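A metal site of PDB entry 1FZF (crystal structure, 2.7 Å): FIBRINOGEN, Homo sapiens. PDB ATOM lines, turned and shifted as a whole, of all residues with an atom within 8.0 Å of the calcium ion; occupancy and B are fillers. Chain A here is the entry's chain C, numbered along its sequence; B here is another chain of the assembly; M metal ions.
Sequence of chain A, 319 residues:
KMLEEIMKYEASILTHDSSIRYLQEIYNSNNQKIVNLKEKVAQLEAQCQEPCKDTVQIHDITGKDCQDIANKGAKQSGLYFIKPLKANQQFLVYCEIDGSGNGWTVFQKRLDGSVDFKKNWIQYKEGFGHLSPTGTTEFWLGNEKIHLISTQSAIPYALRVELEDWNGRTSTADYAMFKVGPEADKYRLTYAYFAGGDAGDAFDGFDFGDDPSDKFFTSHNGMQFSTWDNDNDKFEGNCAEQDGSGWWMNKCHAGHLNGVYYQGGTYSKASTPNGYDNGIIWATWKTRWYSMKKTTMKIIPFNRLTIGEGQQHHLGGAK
OD2 of Asp 214 sits at hydrogen-bond distance from N of Gly 209, at 3.4 Å. OD2 of Asp 211 sits at hydrogen-bond distance from NE2 of His 2 of chain B (3.3 Å). The side-chain carboxylate (OD2) of Asp 211 sits at hydrogen-bond distance from the backbone NH (N) of Asp 214, at 3.4 Å. NE2 of His 2 of chain B lies close to OD1 of Asp 214 (3.4 Å). OG of Ser 213 sits at hydrogen-bond distance from OD1 of Asp 211, 2.9 Å away.
Asp 210 touches the calcium ion (O to CA, 3.2 Å). CA of Pro 212 touches the calcium ion, at 3.9 Å. Asp 214 touches the calcium ion. Within 4 Å of the calcium ion: Asp 207, Gly 209, Asp 210, Asp 211, Pro 212 and Asp 214. The nearest printed residue that does not touch the calcium ion is Phe 208 (4.4 Å).
The calcium ion is bound by OD1 of Asp 207 (2.5 Å), O of Asp 211 (2.6 Å) and O of Gly 209 (2.7 Å). The calcium ion has three donor atoms within binding distance.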
ATOM      1  N   PHE A 206     -11.561 -26.950  -1.180  1.00  0.00           N
ATOM      2  CA  PHE A 206     -10.494 -26.929  -2.165  1.00  0.00           C
ATOM      3  C   PHE A 206      -9.113 -27.135  -1.571  1.00  0.00           C
ATOM      4  O   PHE A 206      -8.787 -26.587  -0.528  1.00  0.00           O
ATOM      5  CB  PHE A 206     -10.535 -25.605  -2.925  1.00  0.00           C
ATOM      6  CG  PHE A 206      -9.641 -25.572  -4.113  1.00  0.00           C
ATOM      7  CD1 PHE A 206     -10.062 -26.129  -5.309  1.00  0.00           C
ATOM      8  CD2 PHE A 206      -8.391 -25.002  -4.043  1.00  0.00           C
ATOM      9  CE1 PHE A 206      -9.234 -26.117  -6.425  1.00  0.00           C
ATOM     10  CE2 PHE A 206      -7.558 -24.978  -5.148  1.00  0.00           C
ATOM     11  CZ  PHE A 206      -7.979 -25.535  -6.344  1.00  0.00           C
ATOM     12  N   ASP A 207      -8.299 -27.935  -2.262  1.00  0.00           N
ATOM     13  CA  ASP A 207      -6.938 -28.230  -1.832  1.00  0.00           C
ATOM     14  C   ASP A 207      -6.090 -27.051  -2.281  1.00  0.00           C
ATOM     15  O   ASP A 207      -5.551 -27.042  -3.402  1.00  0.00           O
ATOM     16  CB  ASP A 207      -6.457 -29.518  -2.508  1.00  0.00           C
ATOM     17  CG  ASP A 207      -5.184 -30.105  -1.860  1.00  0.00           C
ATOM     18  OD1 ASP A 207      -4.358 -29.346  -1.317  1.00  0.00           O
ATOM     19  OD2 ASP A 207      -5.017 -31.348  -1.910  1.00  0.00           O
ATOM     20  N   PHE A 208      -5.982 -26.037  -1.422  1.00  0.00           N
ATOM     21  CA  PHE A 208      -5.209 -24.850  -1.739  1.00  0.00           C
ATOM     22  C   PHE A 208      -3.685 -25.029  -1.570  1.00  0.00           C
ATOM     23  O   PHE A 208      -2.916 -24.070  -1.678  1.00  0.00           O
ATOM     24  CB  PHE A 208      -5.661 -23.681  -0.849  1.00  0.00           C
ATOM     25  CG  PHE A 208      -7.046 -23.134  -1.168  1.00  0.00           C
ATOM     26  CD1 PHE A 208      -7.230 -22.284  -2.263  1.00  0.00           C
ATOM     27  CD2 PHE A 208      -8.141 -23.472  -0.361  1.00  0.00           C
ATOM     28  CE1 PHE A 208      -8.500 -21.768  -2.548  1.00  0.00           C
ATOM     29  CE2 PHE A 208      -9.408 -22.966  -0.646  1.00  0.00           C
ATOM     30  CZ  PHE A 208      -9.586 -22.102  -1.739  1.00  0.00           C
ATOM     31  N   GLY A 209      -3.276 -26.267  -1.338  1.00  0.00           N
ATOM     32  CA  GLY A 209      -1.845 -26.599  -1.172  1.00  0.00           C
ATOM     33  C   GLY A 209      -1.475 -26.627   0.315  1.00  0.00           C
ATOM     34  O   GLY A 209      -2.340 -26.661   1.195  1.00  0.00           O
ATOM     35  N   ASP A 210      -0.176 -26.610   0.558  1.00  0.00           N
ATOM     36  CA  ASP A 210       0.374 -26.649   1.927  1.00  0.00           C
ATOM     37  C   ASP A 210      -0.505 -27.555   2.817  1.00  0.00           C
ATOM     38  O   ASP A 210      -0.922 -28.637   2.394  1.00  0.00           O
ATOM     39  CB  ASP A 210       0.429 -25.237   2.520  1.00  0.00           C
ATOM     40  CG  ASP A 210      -0.911 -24.494   2.439  1.00  0.00           C
ATOM     41  OD1 ASP A 210      -1.255 -23.906   1.353  1.00  0.00           O
ATOM     42  OD2 ASP A 210      -1.689 -24.468   3.471  1.00  0.00           O
ATOM     43  N   ASP A 211      -0.764 -27.050   4.009  1.00  0.00           N
ATOM     44  CA  ASP A 211      -1.571 -27.741   5.051  1.00  0.00           C
ATOM     45  C   ASP A 211      -2.647 -28.681   4.465  1.00  0.00           C
ATOM     46  O   ASP A 211      -3.416 -28.289   3.576  1.00  0.00           O
ATOM     47  CB  ASP A 211      -2.292 -26.706   5.917  1.00  0.00           C
ATOM     48  CG  ASP A 211      -3.345 -27.334   6.828  1.00  0.00           C
ATOM     49  OD1 ASP A 211      -3.034 -28.343   7.574  1.00  0.00           O
ATOM     50  OD2 ASP A 211      -4.544 -26.854   6.854  1.00  0.00           O
ATOM     51  N   PRO A 212      -2.701 -29.945   4.942  1.00  0.00           N
ATOM     52  CA  PRO A 212      -3.677 -30.939   4.499  1.00  0.00           C
ATOM     53  C   PRO A 212      -5.131 -30.606   4.844  1.00  0.00           C
ATOM     54  O   PRO A 212      -6.071 -31.062   4.118  1.00  0.00           O
ATOM     55  CB  PRO A 212      -3.302 -32.201   5.241  1.00  0.00           C
ATOM     56  CG  PRO A 212      -2.116 -31.881   6.138  1.00  0.00           C
ATOM     57  CD  PRO A 212      -1.749 -30.435   5.954  1.00  0.00           C
ATOM     58  N   SER A 213      -5.311 -29.851   5.937  1.00  0.00           N
ATOM     59  CA  SER A 213      -6.664 -29.505   6.466  1.00  0.00           C
ATOM     60  C   SER A 213      -7.434 -28.559   5.541  1.00  0.00           C
ATOM     61  O   SER A 213      -8.635 -28.329   5.735  1.00  0.00           O
ATOM     62  CB  SER A 213      -6.521 -28.811   7.830  1.00  0.00           C
ATOM     63  OG  SER A 213      -5.542 -29.492   8.612  1.00  0.00           O
ATOM     64  N   ASP A 214      -6.731 -28.011   4.565  1.00  0.00           N
ATOM     65  CA  ASP A 214      -7.282 -27.081   3.577  1.00  0.00           C
ATOM     66  C   ASP A 214      -8.642 -27.422   3.011  1.00  0.00           C
ATOM     67  O   ASP A 214      -9.617 -26.731   3.267  1.00  0.00           O
ATOM     68  CB  ASP A 214      -6.320 -26.946   2.398  1.00  0.00           C
ATOM     69  CG  ASP A 214      -5.172 -26.043   2.700  1.00  0.00           C
ATOM     70  OD1 ASP A 214      -4.874 -25.842   3.898  1.00  0.00           O
ATOM     71  OD2 ASP A 214      -4.572 -25.513   1.741  1.00  0.00           O
ATOM     72  N   LYS A 215      -8.687 -28.475   2.200  1.00  0.00           N
ATOM     73  CA  LYS A 215      -9.935 -28.893   1.577  1.00  0.00           C
ATOM     74  C   LYS A 215     -11.028 -29.115   2.608  1.00  0.00           C
ATOM     75  O   LYS A 215     -12.168 -28.708   2.388  1.00  0.00           O
ATOM     76  CB  LYS A 215      -9.704 -30.144   0.719  1.00  0.00           C
ATOM     77  CG  LYS A 215     -10.859 -30.476  -0.214  1.00  0.00           C
ATOM     78  CD  LYS A 215     -10.522 -31.605  -1.169  1.00  0.00           C
ATOM     79  CE  LYS A 215     -11.683 -31.917  -2.113  1.00  0.00           C
ATOM     80  NZ  LYS A 215     -12.908 -32.393  -1.394  1.00  0.00           N
ATOM     81  N   PHE A 216     -10.681 -29.700   3.745  1.00  0.00           N
ATOM     82  CA  PHE A 216     -11.662 -29.942   4.799  1.00  0.00           C
ATOM     83  C   PHE A 216     -12.190 -28.623   5.339  1.00  0.00           C
ATOM     84  O   PHE A 216     -13.400 -28.442   5.491  1.00  0.00           O
ATOM     85  CB  PHE A 216     -11.045 -30.756   5.938  1.00  0.00           C
ATOM     86  CG  PHE A 216     -11.887 -30.779   7.193  1.00  0.00           C
ATOM     87  CD1 PHE A 216     -13.168 -31.315   7.180  1.00  0.00           C
ATOM     88  CD2 PHE A 216     -11.401 -30.219   8.377  1.00  0.00           C
ATOM     89  CE1 PHE A 216     -13.961 -31.290   8.330  1.00  0.00           C
ATOM     90  CE2 PHE A 216     -12.193 -30.194   9.528  1.00  0.00           C
ATOM     91  CZ  PHE A 216     -13.473 -30.730   9.504  1.00  0.00           C
ATOM     92  N   HIS B   2      -8.724 -20.240   2.647  1.00  0.00           N
ATOM     93  CA  HIS B   2      -8.303 -20.932   3.863  1.00  0.00           C
ATOM     94  C   HIS B   2      -7.758 -19.961   4.876  1.00  0.00           C
ATOM     95  O   HIS B   2      -7.093 -18.965   4.545  1.00  0.00           O
ATOM     96  CB  HIS B   2      -7.245 -22.000   3.573  1.00  0.00           C
ATOM     97  CG  HIS B   2      -6.861 -22.792   4.784  1.00  0.00           C
ATOM     98  ND1 HIS B   2      -7.779 -23.449   5.570  1.00  0.00           N
ATOM     99  CD2 HIS B   2      -5.650 -23.020   5.346  1.00  0.00           C
ATOM    100  CE1 HIS B   2      -7.154 -24.063   6.560  1.00  0.00           C
ATOM    101  NE2 HIS B   2      -5.864 -23.817   6.442  1.00  0.00           N
HETATM  102 CA    CA M   1      -3.814 -28.907   1.123  1.00  0.00          CA
